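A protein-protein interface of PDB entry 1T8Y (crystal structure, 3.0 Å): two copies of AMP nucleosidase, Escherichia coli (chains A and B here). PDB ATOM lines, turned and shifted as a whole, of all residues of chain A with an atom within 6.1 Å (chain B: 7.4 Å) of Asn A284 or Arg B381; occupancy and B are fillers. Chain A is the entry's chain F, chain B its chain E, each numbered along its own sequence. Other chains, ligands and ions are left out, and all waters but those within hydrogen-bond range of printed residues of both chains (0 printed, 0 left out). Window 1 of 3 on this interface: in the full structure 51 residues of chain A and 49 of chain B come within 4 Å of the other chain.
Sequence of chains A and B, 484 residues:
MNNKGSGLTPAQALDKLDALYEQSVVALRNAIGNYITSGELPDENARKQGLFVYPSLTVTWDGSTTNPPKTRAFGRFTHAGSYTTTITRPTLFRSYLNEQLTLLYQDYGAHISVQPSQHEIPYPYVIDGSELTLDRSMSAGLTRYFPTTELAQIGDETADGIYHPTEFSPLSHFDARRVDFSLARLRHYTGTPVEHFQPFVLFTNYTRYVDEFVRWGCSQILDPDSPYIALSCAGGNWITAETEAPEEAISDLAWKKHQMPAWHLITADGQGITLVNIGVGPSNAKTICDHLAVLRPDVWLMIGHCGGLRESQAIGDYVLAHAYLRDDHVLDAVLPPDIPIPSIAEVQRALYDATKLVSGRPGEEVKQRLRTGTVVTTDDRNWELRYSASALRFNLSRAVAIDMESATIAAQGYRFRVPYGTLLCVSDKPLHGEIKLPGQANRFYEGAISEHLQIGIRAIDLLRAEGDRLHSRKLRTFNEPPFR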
ATOM      1  N   TYR A 189      -2.945 -22.690   2.068  1.00  0.00           N
ATOM      2  CA  TYR A 189      -4.303 -23.174   2.342  1.00  0.00           C
ATOM      3  C   TYR A 189      -4.326 -24.643   2.731  1.00  0.00           C
ATOM      4  O   TYR A 189      -5.045 -25.056   3.641  1.00  0.00           O
ATOM      5  CB  TYR A 189      -5.228 -22.993   1.115  1.00  0.00           C
ATOM      6  CG  TYR A 189      -5.526 -21.560   0.715  1.00  0.00           C
ATOM      7  CD1 TYR A 189      -5.997 -20.631   1.646  1.00  0.00           C
ATOM      8  CD2 TYR A 189      -5.332 -21.127  -0.598  1.00  0.00           C
ATOM      9  CE1 TYR A 189      -6.264 -19.298   1.276  1.00  0.00           C
ATOM     10  CE2 TYR A 189      -5.597 -19.798  -0.977  1.00  0.00           C
ATOM     11  CZ  TYR A 189      -6.059 -18.893  -0.034  1.00  0.00           C
ATOM     12  OH  TYR A 189      -6.295 -17.586  -0.400  1.00  0.00           O
ATOM     13  N   GLN A 259      -7.226 -23.311   6.055  1.00  0.00           N
ATOM     14  CA  GLN A 259      -8.616 -23.231   5.625  1.00  0.00           C
ATOM     15  C   GLN A 259      -9.090 -24.420   4.785  1.00  0.00           C
ATOM     16  O   GLN A 259     -10.292 -24.638   4.637  1.00  0.00           O
ATOM     17  CB  GLN A 259      -8.821 -21.935   4.851  1.00  0.00           C
ATOM     18  CG  GLN A 259      -8.373 -20.717   5.620  1.00  0.00           C
ATOM     19  CD  GLN A 259      -8.368 -19.475   4.761  1.00  0.00           C
ATOM     20  OE1 GLN A 259      -9.372 -19.149   4.117  1.00  0.00           O
ATOM     21  NE2 GLN A 259      -7.236 -18.769   4.743  1.00  0.00           N
ATOM     22  N   MET A 260      -8.157 -25.184   4.228  1.00  0.00           N
ATOM     23  CA  MET A 260      -8.518 -26.349   3.432  1.00  0.00           C
ATOM     24  C   MET A 260      -7.414 -27.372   3.475  1.00  0.00           C
ATOM     25  O   MET A 260      -6.633 -27.513   2.532  1.00  0.00           O
ATOM     26  CB  MET A 260      -8.783 -25.964   1.990  1.00  0.00           C
ATOM     27  CG  MET A 260     -10.004 -25.079   1.813  1.00  0.00           C
ATOM     28  SD  MET A 260      -9.808 -23.819   0.296  1.00  0.00           S
ATOM     29  CE  MET A 260      -8.779 -22.347   1.189  1.00  0.00           C
ATOM     30  N   ASN A 277     -10.143 -31.091   2.123  1.00  0.00           N
ATOM     31  CA  ASN A 277     -11.400 -30.805   2.785  1.00  0.00           C
ATOM     32  C   ASN A 277     -11.630 -29.319   2.550  1.00  0.00           C
ATOM     33  O   ASN A 277     -11.155 -28.474   3.315  1.00  0.00           O
ATOM     34  CB  ASN A 277     -11.316 -31.081   4.273  1.00  0.00           C
ATOM     35  CG  ASN A 277     -12.614 -30.811   4.962  1.00  0.00           C
ATOM     36  OD1 ASN A 277     -13.624 -31.444   4.663  1.00  0.00           O
ATOM     37  ND2 ASN A 277     -12.611 -29.856   5.880  1.00  0.00           N
ATOM     38  N   ILE A 278     -12.350 -29.017   1.475  1.00  0.00           N
ATOM     39  CA  ILE A 278     -12.624 -27.648   1.073  1.00  0.00           C
ATOM     40  C   ILE A 278     -13.532 -26.890   2.024  1.00  0.00           C
ATOM     41  O   ILE A 278     -13.659 -25.665   1.937  1.00  0.00           O
ATOM     42  CB  ILE A 278     -13.217 -27.612  -0.353  1.00  0.00           C
ATOM     43  CG1 ILE A 278     -14.533 -28.408  -0.406  1.00  0.00           C
ATOM     44  CG2 ILE A 278     -12.185 -28.164  -1.333  1.00  0.00           C
ATOM     45  CD1 ILE A 278     -15.120 -28.605  -1.808  1.00  0.00           C
ATOM     46  N   GLY A 279     -14.153 -27.601   2.952  1.00  0.00           N
ATOM     47  CA  GLY A 279     -15.021 -26.911   3.880  1.00  0.00           C
ATOM     48  C   GLY A 279     -16.265 -26.496   3.137  1.00  0.00           C
ATOM     49  O   GLY A 279     -16.551 -27.067   2.081  1.00  0.00           O
ATOM     50  N   VAL A 280     -16.988 -25.501   3.654  1.00  0.00           N
ATOM     51  CA  VAL A 280     -18.234 -25.069   3.020  1.00  0.00           C
ATOM     52  C   VAL A 280     -18.246 -23.617   2.520  1.00  0.00           C
ATOM     53  O   VAL A 280     -17.707 -22.703   3.165  1.00  0.00           O
ATOM     54  CB  VAL A 280     -19.477 -25.367   3.975  1.00  0.00           C
ATOM     55  CG1 VAL A 280     -20.699 -24.507   3.598  1.00  0.00           C
ATOM     56  CG2 VAL A 280     -19.868 -26.851   3.871  1.00  0.00           C
ATOM     57  N   GLY A 281     -18.871 -23.451   1.348  1.00  0.00           N
ATOM     58  CA  GLY A 281     -18.995 -22.168   0.680  1.00  0.00           C
ATOM     59  C   GLY A 281     -18.454 -22.268  -0.742  1.00  0.00           C
ATOM     60  O   GLY A 281     -17.421 -22.893  -0.939  1.00  0.00           O
ATOM     61  N   PRO A 282     -19.122 -21.692  -1.760  1.00  0.00           N
ATOM     62  CA  PRO A 282     -18.594 -21.787  -3.131  1.00  0.00           C
ATOM     63  C   PRO A 282     -17.331 -20.953  -3.273  1.00  0.00           C
ATOM     64  O   PRO A 282     -16.481 -21.226  -4.119  1.00  0.00           O
ATOM     65  CB  PRO A 282     -19.743 -21.253  -3.986  1.00  0.00           C
ATOM     66  CG  PRO A 282     -20.946 -21.602  -3.189  1.00  0.00           C
ATOM     67  CD  PRO A 282     -20.516 -21.217  -1.784  1.00  0.00           C
ATOM     68  N   SER A 283     -17.233 -19.935  -2.424  1.00  0.00           N
ATOM     69  CA  SER A 283     -16.091 -19.033  -2.402  1.00  0.00           C
ATOM     70  C   SER A 283     -14.830 -19.877  -2.236  1.00  0.00           C
ATOM     71  O   SER A 283     -13.831 -19.683  -2.930  1.00  0.00           O
ATOM     72  CB  SER A 283     -16.240 -18.057  -1.234  1.00  0.00           C
ATOM     73  OG  SER A 283     -17.592 -17.636  -1.099  1.00  0.00           O
ATOM     74  N   ASN A 284     -14.902 -20.839  -1.327  1.00  0.00           N
ATOM     75  CA  ASN A 284     -13.786 -21.721  -1.056  1.00  0.00           C
ATOM     76  C   ASN A 284     -13.483 -22.697  -2.155  1.00  0.00           C
ATOM     77  O   ASN A 284     -12.333 -22.926  -2.470  1.00  0.00           O
ATOM     78  CB  ASN A 284     -14.043 -22.503   0.212  1.00  0.00           C
ATOM     79  CG  ASN A 284     -13.124 -22.098   1.316  1.00  0.00           C
ATOM     80  OD1 ASN A 284     -12.807 -22.901   2.194  1.00  0.00           O
ATOM     81  ND2 ASN A 284     -12.683 -20.840   1.290  1.00  0.00           N
ATOM     82  N   ALA A 285     -14.521 -23.290  -2.719  1.00  0.00           N
ATOM     83  CA  ALA A 285     -14.345 -24.261  -3.783  1.00  0.00           C
ATOM     84  C   ALA A 285     -13.673 -23.617  -4.985  1.00  0.00           C
ATOM     85  O   ALA A 285     -12.870 -24.254  -5.670  1.00  0.00           O
ATOM     86  CB  ALA A 285     -15.691 -24.858  -4.184  1.00  0.00           C
ATOM     87  N   LYS A 286     -13.996 -22.356  -5.253  1.00  0.00           N
ATOM     88  CA  LYS A 286     -13.375 -21.693  -6.386  1.00  0.00           C
ATOM     89  C   LYS A 286     -11.898 -21.471  -6.100  1.00  0.00           C
ATOM     90  O   LYS A 286     -11.027 -21.836  -6.901  1.00  0.00           O
ATOM     91  CB  LYS A 286     -14.021 -20.338  -6.675  1.00  0.00           C
ATOM     92  CG  LYS A 286     -13.297 -19.620  -7.810  1.00  0.00           C
ATOM     93  CD  LYS A 286     -13.862 -18.266  -8.146  1.00  0.00           C
ATOM     94  CE  LYS A 286     -13.022 -17.591  -9.230  1.00  0.00           C
ATOM     95  NZ  LYS A 286     -11.645 -17.289  -8.769  1.00  0.00           N
ATOM     96  N   THR A 287     -11.629 -20.868  -4.948  1.00  0.00           N
ATOM     97  CA  THR A 287     -10.262 -20.572  -4.539  1.00  0.00           C
ATOM     98  C   THR A 287      -9.341 -21.786  -4.638  1.00  0.00           C
ATOM     99  O   THR A 287      -8.296 -21.721  -5.279  1.00  0.00           O
ATOM    100  CB  THR A 287     -10.193 -20.035  -3.084  1.00  0.00           C
ATOM    101  OG1 THR A 287     -10.946 -18.820  -2.959  1.00  0.00           O
ATOM    102  CG2 THR A 287      -8.764 -19.755  -2.712  1.00  0.00           C
ATOM    103  N   ILE A 288      -9.717 -22.892  -4.008  1.00  0.00           N
ATOM    104  CA  ILE A 288      -8.883 -24.072  -4.052  1.00  0.00           C
ATOM    105  C   ILE A 288      -8.614 -24.600  -5.477  1.00  0.00           C
ATOM    106  O   ILE A 288      -7.487 -24.973  -5.799  1.00  0.00           O
ATOM    107  CB  ILE A 288      -9.482 -25.191  -3.173  1.00  0.00           C
ATOM    108  CG1 ILE A 288      -8.415 -26.258  -2.916  1.00  0.00           C
ATOM    109  CG2 ILE A 288     -10.703 -25.798  -3.842  1.00  0.00           C
ATOM    110  CD1 ILE A 288      -7.220 -25.747  -2.119  1.00  0.00           C
ATOM    111  N   CYS A 289      -9.625 -24.619  -6.342  1.00  0.00           N
ATOM    112  CA  CYS A 289      -9.421 -25.133  -7.696  1.00  0.00           C
ATOM    113  C   CYS A 289      -8.565 -24.212  -8.523  1.00  0.00           C
ATOM    114  O   CYS A 289      -7.830 -24.668  -9.394  1.00  0.00           O
ATOM    115  CB  CYS A 289     -10.755 -25.379  -8.399  1.00  0.00           C
ATOM    116  SG  CYS A 289     -11.700 -26.769  -7.732  1.00  0.00           S
ATOM    117  N   VAL A 330     -20.373 -17.204  -7.579  1.00  0.00           N
ATOM    118  CA  VAL A 330     -18.934 -17.011  -7.602  1.00  0.00           C
ATOM    119  C   VAL A 330     -18.228 -17.122  -8.949  1.00  0.00           C
ATOM    120  O   VAL A 330     -17.162 -16.542  -9.115  1.00  0.00           O
ATOM    121  CB  VAL A 330     -18.266 -17.959  -6.583  1.00  0.00           C
ATOM    122  CG1 VAL A 330     -18.218 -19.393  -7.136  1.00  0.00           C
ATOM    123  CG2 VAL A 330     -16.902 -17.431  -6.217  1.00  0.00           C
ATOM    124  N   ASN B 205     -12.110 -12.086  10.930  1.00  0.00           N
ATOM    125  CA  ASN B 205     -11.816 -13.047   9.877  1.00  0.00           C
ATOM    126  C   ASN B 205     -10.434 -13.643  10.017  1.00  0.00           C
ATOM    127  O   ASN B 205      -9.953 -14.321   9.107  1.00  0.00           O
ATOM    128  CB  ASN B 205     -11.944 -12.397   8.482  1.00  0.00           C
ATOM    129  CG  ASN B 205     -11.224 -11.046   8.373  1.00  0.00           C
ATOM    130  OD1 ASN B 205     -10.162 -10.830   8.953  1.00  0.00           O
ATOM    131  ND2 ASN B 205     -11.803 -10.139   7.605  1.00  0.00           N
ATOM    132  N   GLY B 279     -14.601 -16.338  10.013  1.00  0.00           N
ATOM    133  CA  GLY B 279     -13.785 -16.972   8.999  1.00  0.00           C
ATOM    134  C   GLY B 279     -13.916 -16.191   7.714  1.00  0.00           C
ATOM    135  O   GLY B 279     -14.296 -15.020   7.759  1.00  0.00           O
ATOM    136  N   VAL B 280     -13.636 -16.815   6.572  1.00  0.00           N
ATOM    137  CA  VAL B 280     -13.705 -16.095   5.296  1.00  0.00           C
ATOM    138  C   VAL B 280     -14.756 -16.596   4.300  1.00  0.00           C
ATOM    139  O   VAL B 280     -14.982 -17.804   4.153  1.00  0.00           O
ATOM    140  CB  VAL B 280     -12.280 -16.039   4.612  1.00  0.00           C
ATOM    141  CG1 VAL B 280     -12.390 -15.673   3.117  1.00  0.00           C
ATOM    142  CG2 VAL B 280     -11.405 -14.995   5.332  1.00  0.00           C
ATOM    143  N   GLY B 281     -15.388 -15.632   3.626  1.00  0.00           N
ATOM    144  CA  GLY B 281     -16.423 -15.920   2.647  1.00  0.00           C
ATOM    145  C   GLY B 281     -17.707 -15.173   2.985  1.00  0.00           C
ATOM    146  O   GLY B 281     -18.096 -15.140   4.157  1.00  0.00           O
ATOM    147  N   SER B 283     -20.574 -16.026   2.158  1.00  0.00           N
ATOM    148  CA  SER B 283     -21.509 -17.097   2.432  1.00  0.00           C
ATOM    149  C   SER B 283     -21.613 -17.261   3.945  1.00  0.00           C
ATOM    150  O   SER B 283     -22.707 -17.369   4.506  1.00  0.00           O
ATOM    151  CB  SER B 283     -20.999 -18.376   1.770  1.00  0.00           C
ATOM    152  OG  SER B 283     -20.386 -18.072   0.515  1.00  0.00           O
ATOM    153  N   HIS B 305      -9.117  -8.061   8.574  1.00  0.00           N
ATOM    154  CA  HIS B 305      -8.090  -7.585   7.664  1.00  0.00           C
ATOM    155  C   HIS B 305      -8.682  -7.276   6.305  1.00  0.00           C
ATOM    156  O   HIS B 305      -9.813  -7.651   6.005  1.00  0.00           O
ATOM    157  CB  HIS B 305      -6.995  -8.639   7.521  1.00  0.00           C
ATOM    158  CG  HIS B 305      -7.464  -9.912   6.896  1.00  0.00           C
ATOM    159  ND1 HIS B 305      -7.785 -10.009   5.560  1.00  0.00           N
ATOM    160  CD2 HIS B 305      -7.674 -11.139   7.426  1.00  0.00           C
ATOM    161  CE1 HIS B 305      -8.174 -11.243   5.292  1.00  0.00           C
ATOM    162  NE2 HIS B 305      -8.115 -11.949   6.409  1.00  0.00           N
ATOM    163  N   THR B 378     -16.041  -8.941  -1.764  1.00  0.00           N
ATOM    164  CA  THR B 378     -16.188  -9.877  -2.874  1.00  0.00           C
ATOM    165  C   THR B 378     -16.200 -11.334  -2.446  1.00  0.00           C
ATOM    166  O   THR B 378     -15.670 -11.687  -1.403  1.00  0.00           O
ATOM    167  CB  THR B 378     -15.034  -9.704  -3.891  1.00  0.00           C
ATOM    168  OG1 THR B 378     -15.137 -10.699  -4.910  1.00  0.00           O
ATOM    169  CG2 THR B 378     -13.696  -9.889  -3.217  1.00  0.00           C
ATOM    170  N   ASP B 379     -16.789 -12.184  -3.270  1.00  0.00           N
ATOM    171  CA  ASP B 379     -16.831 -13.598  -2.955  1.00  0.00           C
ATOM    172  C   ASP B 379     -15.755 -14.338  -3.742  1.00  0.00           C
ATOM    173  O   ASP B 379     -15.593 -15.557  -3.619  1.00  0.00           O
ATOM    174  CB  ASP B 379     -18.218 -14.160  -3.273  1.00  0.00           C
ATOM    175  CG  ASP B 379     -18.551 -14.120  -4.758  1.00  0.00           C
ATOM    176  OD1 ASP B 379     -17.826 -13.461  -5.537  1.00  0.00           O
ATOM    177  OD2 ASP B 379     -19.555 -14.753  -5.143  1.00  0.00           O
ATOM    178  N   ASP B 380     -15.019 -13.593  -4.556  1.00  0.00           N
ATOM    179  CA  ASP B 380     -13.948 -14.169  -5.355  1.00  0.00           C
ATOM    180  C   ASP B 380     -12.632 -13.754  -4.724  1.00  0.00           C
ATOM    181  O   ASP B 380     -12.169 -12.634  -4.923  1.00  0.00           O
ATOM    182  CB  ASP B 380     -14.026 -13.670  -6.798  1.00  0.00           C
ATOM    183  CG  ASP B 380     -12.843 -14.101  -7.633  1.00  0.00           C
ATOM    184  OD1 ASP B 380     -12.184 -15.076  -7.240  1.00  0.00           O
ATOM    185  OD2 ASP B 380     -12.577 -13.482  -8.689  1.00  0.00           O
ATOM    186  N   ARG B 381     -12.040 -14.655  -3.943  1.00  0.00           N
ATOM    187  CA  ARG B 381     -10.774 -14.360  -3.289  1.00  0.00           C
ATOM    188  C   ARG B 381      -9.608 -14.119  -4.253  1.00  0.00           C
ATOM    189  O   ARG B 381      -8.743 -13.292  -3.972  1.00  0.00           O
ATOM    190  CB  ARG B 381     -10.397 -15.469  -2.334  1.00  0.00           C
ATOM    191  CG  ARG B 381      -8.988 -15.341  -1.853  1.00  0.00           C
ATOM    192  CD  ARG B 381      -8.949 -15.555  -0.377  1.00  0.00           C
ATOM    193  NE  ARG B 381      -9.698 -16.750   0.017  1.00  0.00           N
ATOM    194  CZ  ARG B 381      -9.734 -17.235   1.258  1.00  0.00           C
ATOM    195  NH1 ARG B 381      -9.063 -16.625   2.239  1.00  0.00           N
ATOM    196  NH2 ARG B 381     -10.431 -18.337   1.514  1.00  0.00           N
ATOM    197  N   ASN B 382      -9.555 -14.846  -5.367  1.00  0.00           N
ATOM    198  CA  ASN B 382      -8.485 -14.620  -6.335  1.00  0.00           C
ATOM    199  C   ASN B 382      -8.950 -13.578  -7.349  1.00  0.00           C
ATOM    200  O   ASN B 382      -8.826 -13.762  -8.564  1.00  0.00           O
ATOM    201  CB  ASN B 382      -8.121 -15.908  -7.061  1.00  0.00           C
ATOM    202  CG  ASN B 382      -7.614 -16.978  -6.126  1.00  0.00           C
ATOM    203  OD1 ASN B 382      -6.852 -16.711  -5.184  1.00  0.00           O
ATOM    204  ND2 ASN B 382      -8.022 -18.211  -6.384  1.00  0.00           N
ATOM    205  N   TRP B 383      -9.498 -12.480  -6.842  1.00  0.00           N
ATOM    206  CA  TRP B 383      -9.987 -11.430  -7.713  1.00  0.00           C
ATOM    207  C   TRP B 383      -8.847 -10.777  -8.471  1.00  0.00           C
ATOM    208  O   TRP B 383      -9.051 -10.234  -9.543  1.00  0.00           O
ATOM    209  CB  TRP B 383     -10.742 -10.377  -6.907  1.00  0.00           C
ATOM    210  CG  TRP B 383      -9.922  -9.721  -5.867  1.00  0.00           C
ATOM    211  CD1 TRP B 383      -9.801 -10.091  -4.566  1.00  0.00           C
ATOM    212  CD2 TRP B 383      -9.031  -8.622  -6.058  1.00  0.00           C
ATOM    213  NE1 TRP B 383      -8.881  -9.295  -3.924  1.00  0.00           N
ATOM    214  CE2 TRP B 383      -8.391  -8.383  -4.821  1.00  0.00           C
ATOM    215  CE3 TRP B 383      -8.704  -7.821  -7.158  1.00  0.00           C
ATOM    216  CZ2 TRP B 383      -7.441  -7.376  -4.652  1.00  0.00           C
ATOM    217  CZ3 TRP B 383      -7.757  -6.816  -6.993  1.00  0.00           C
ATOM    218  CH2 TRP B 383      -7.137  -6.603  -5.747  1.00  0.00           C
ATOM    219  N   GLU B 384      -7.645 -10.827  -7.913  1.00  0.00           N
ATOM    220  CA  GLU B 384      -6.489 -10.229  -8.564  1.00  0.00           C
ATOM    221  C   GLU B 384      -6.314 -10.832  -9.941  1.00  0.00           C
ATOM    222  O   GLU B 384      -5.852 -10.171 -10.856  1.00  0.00           O
ATOM    223  CB  GLU B 384      -5.206 -10.479  -7.765  1.00  0.00           C
ATOM    224  CG  GLU B 384      -5.240  -9.980  -6.337  1.00  0.00           C
ATOM    225  CD  GLU B 384      -5.670 -11.044  -5.331  1.00  0.00           C
ATOM    226  OE1 GLU B 384      -6.597 -11.823  -5.653  1.00  0.00           O
ATOM    227  OE2 GLU B 384      -5.089 -11.087  -4.212  1.00  0.00           O
ATOM    228  N   LEU B 385      -6.678 -12.096 -10.091  1.00  0.00           N
ATOM    229  CA  LEU B 385      -6.523 -12.752 -11.374  1.00  0.00           C
ATOM    230  C   LEU B 385      -7.397 -12.109 -12.443  1.00  0.00           C
ATOM    231  O   LEU B 385      -7.305 -12.470 -13.606  1.00  0.00           O
ATOM    232  CB  LEU B 385      -6.849 -14.243 -11.253  1.00  0.00           C
ATOM    233  CG  LEU B 385      -5.924 -15.136 -10.416  1.00  0.00           C
ATOM    234  CD1 LEU B 385      -6.473 -16.535 -10.410  1.00  0.00           C
ATOM    235  CD2 LEU B 385      -4.532 -15.152 -10.964  1.00  0.00           C
ATOM    236  N   ILE B 402     -10.398  -3.756   0.001  1.00  0.00           N
ATOM    237  CA  ILE B 402     -11.247  -4.871  -0.427  1.00  0.00           C
ATOM    238  C   ILE B 402     -11.197  -6.041   0.582  1.00  0.00           C
ATOM    239  O   ILE B 402     -10.149  -6.345   1.139  1.00  0.00           O
ATOM    240  CB  ILE B 402     -10.834  -5.342  -1.837  1.00  0.00           C
ATOM    241  CG1 ILE B 402     -11.655  -6.567  -2.245  1.00  0.00           C
ATOM    242  CG2 ILE B 402      -9.340  -5.593  -1.880  1.00  0.00           C
ATOM    243  CD1 ILE B 402     -11.495  -6.968  -3.706  1.00  0.00           C
ATOM    244  N   MET B 404     -13.861  -9.639   2.285  1.00  0.00           N
ATOM    245  CA  MET B 404     -14.897 -10.627   1.959  1.00  0.00           C
ATOM    246  C   MET B 404     -16.048 -10.837   2.959  1.00  0.00           C
ATOM    247  O   MET B 404     -16.701 -11.875   2.938  1.00  0.00           O
ATOM    248  CB  MET B 404     -14.233 -11.973   1.670  1.00  0.00           C
ATOM    249  CG  MET B 404     -13.157 -11.875   0.598  1.00  0.00           C
ATOM    250  SD  MET B 404     -12.439 -13.685   0.014  1.00  0.00           S
ATOM    251  CE  MET B 404     -14.063 -14.435  -0.949  1.00  0.00           C
ATOM    252  N   GLU B 405     -16.310  -9.856   3.816  1.00  0.00           N
ATOM    253  CA  GLU B 405     -17.389  -9.985   4.788  1.00  0.00           C
ATOM    254  C   GLU B 405     -18.087  -8.657   5.093  1.00  0.00           C
ATOM    255  O   GLU B 405     -19.299  -8.636   5.297  1.00  0.00           O
ATOM    256  CB  GLU B 405     -16.865 -10.586   6.102  1.00  0.00           C
ATOM    257  CG  GLU B 405     -16.409 -12.048   6.041  1.00  0.00           C
ATOM    258  CD  GLU B 405     -14.990 -12.219   5.495  1.00  0.00           C
ATOM    259  OE1 GLU B 405     -14.150 -11.324   5.760  1.00  0.00           O
ATOM    260  OE2 GLU B 405     -14.712 -13.251   4.824  1.00  0.00           O
ATOM    261  N   LEU B 437      -0.334 -13.144   2.482  1.00  0.00           N
ATOM    262  CA  LEU B 437      -1.514 -13.899   2.911  1.00  0.00           C
ATOM    263  C   LEU B 437      -1.635 -13.925   4.442  1.00  0.00           C
ATOM    264  O   LEU B 437      -0.627 -13.913   5.161  1.00  0.00           O
ATOM    265  CB  LEU B 437      -1.441 -15.339   2.389  1.00  0.00           C
ATOM    266  CG  LEU B 437      -1.175 -15.500   0.891  1.00  0.00           C
ATOM    267  CD1 LEU B 437      -0.895 -16.960   0.599  1.00  0.00           C
ATOM    268  CD2 LEU B 437      -2.364 -14.998   0.078  1.00  0.00           C
ATOM    269  N   PRO B 438      -2.876 -13.935   4.962  1.00  0.00           N
ATOM    270  CA  PRO B 438      -3.029 -13.969   6.417  1.00  0.00           C
ATOM    271  C   PRO B 438      -2.359 -15.229   6.941  1.00  0.00           C
ATOM    272  O   PRO B 438      -2.749 -16.339   6.574  1.00  0.00           O
ATOM    273  CB  PRO B 438      -4.541 -13.992   6.598  1.00  0.00           C
ATOM    274  CG  PRO B 438      -5.018 -13.179   5.436  1.00  0.00           C
ATOM    275  CD  PRO B 438      -4.180 -13.741   4.307  1.00  0.00           C
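OG of Ser B283 sits at hydrogen-bond distance from OG of Ser A283 (3.3 Å).
The side-chain amino group (NZ) of Lys A286 is in salt-bridge range of the side-chain carboxylate (OD1) of Asp B380 (2.7 Å).
NH2 of Arg B381 lies within hydrogen-bond range of OE1 of Gln A259 (2.9 Å).
ND2 of Asn A284 sits close to NH2 of Arg B381, 3.4 Å away.
The side-chain hydroxyl (OG1) of Thr B378 is in hydrogen-bond range of the backbone NH (N) of Asp B380, at 2.9 Å.
OD1 of Asp B380 sits at hydrogen-bond distance from N of Asn B382 (3.2 Å).
The backbone carbonyl oxygen (O) of Tyr A189 sits at hydrogen-bond distance from the backbone NH (N) of Met A260 (3.2 Å).
SD of Met A260 lies close to OD1 of Asn A284, 3.7 Å away.
The backbone carbonyl oxygen (O) of Ile A278 sits close to the side-chain amide oxygen (OD1) of Asn A284, 2.9 Å away.
The side-chain hydroxyl (OG1) of Thr A287 is in hydrogen-bond range of the backbone carbonyl oxygen (O) of Ser A283, at 3.0 Å.
Among the printed residues, merely in contact across the chains: Tyr A189 with Arg B381 (3.3 Å), Val A330 with Asp B379 (3.4 Å), Thr A287 with Arg B381 (3.5 Å), Ser A283 with Asp B379 (3.5 Å), Thr A287 with Asn B382 (3.7 Å) and Pro A282 with Ser B283 (3.9 Å).
Arg B381 touches just these residues of chain A: Tyr A189 (3.3 Å), Gln A259 (2.9 Å), Asn A284 (3.4 Å) and Thr A287 (3.5 Å).
Of the printed residues of chain B, Ser A283 touches Ser B283 (3.3 Å) and Asp B379 (3.5 Å).
Printed residues of chain A within 4 Å of Asp B380: Lys A286.
Of the printed residues of chain B, Val A330 touches Asp B379 (3.4 Å).
Trp B383 touches none of the printed residues of chain A.
The nearest residue of chain B that does not touch Asn A284 is Val B280 (4.8 Å).
The nearest residue of chain A that does not touch Arg B381 is Met A260 (4.3 Å).
The nearest printed residue of chain B that does not touch Val A330 is Asp B380 (4.5 Å).
Of the 17 printed residues of chain A, 8 touch a printed residue of chain B.
Hydrophobic or aromatic side chains of chain A that line the printed part of chain B: Tyr A189, Pro A282 and Val A330.
Along chain A the printed residues that touch a printed residue of chain B span positions 189 to 330.
Among the printed residues, Asp or Glu carboxylates within 4 Å of a Lys or Arg side-chain nitrogen of the other chain: Lys A286 with Asp B380 (2.7 Å).
Ser B283 touches its own counterpart, Ser A283.
Positions printed for both chains: 279, 280, 281 and 283.
Of the 10 pairs that touch across the chains among the printed residues, 1 has its exchanged pair printed and touching as well.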
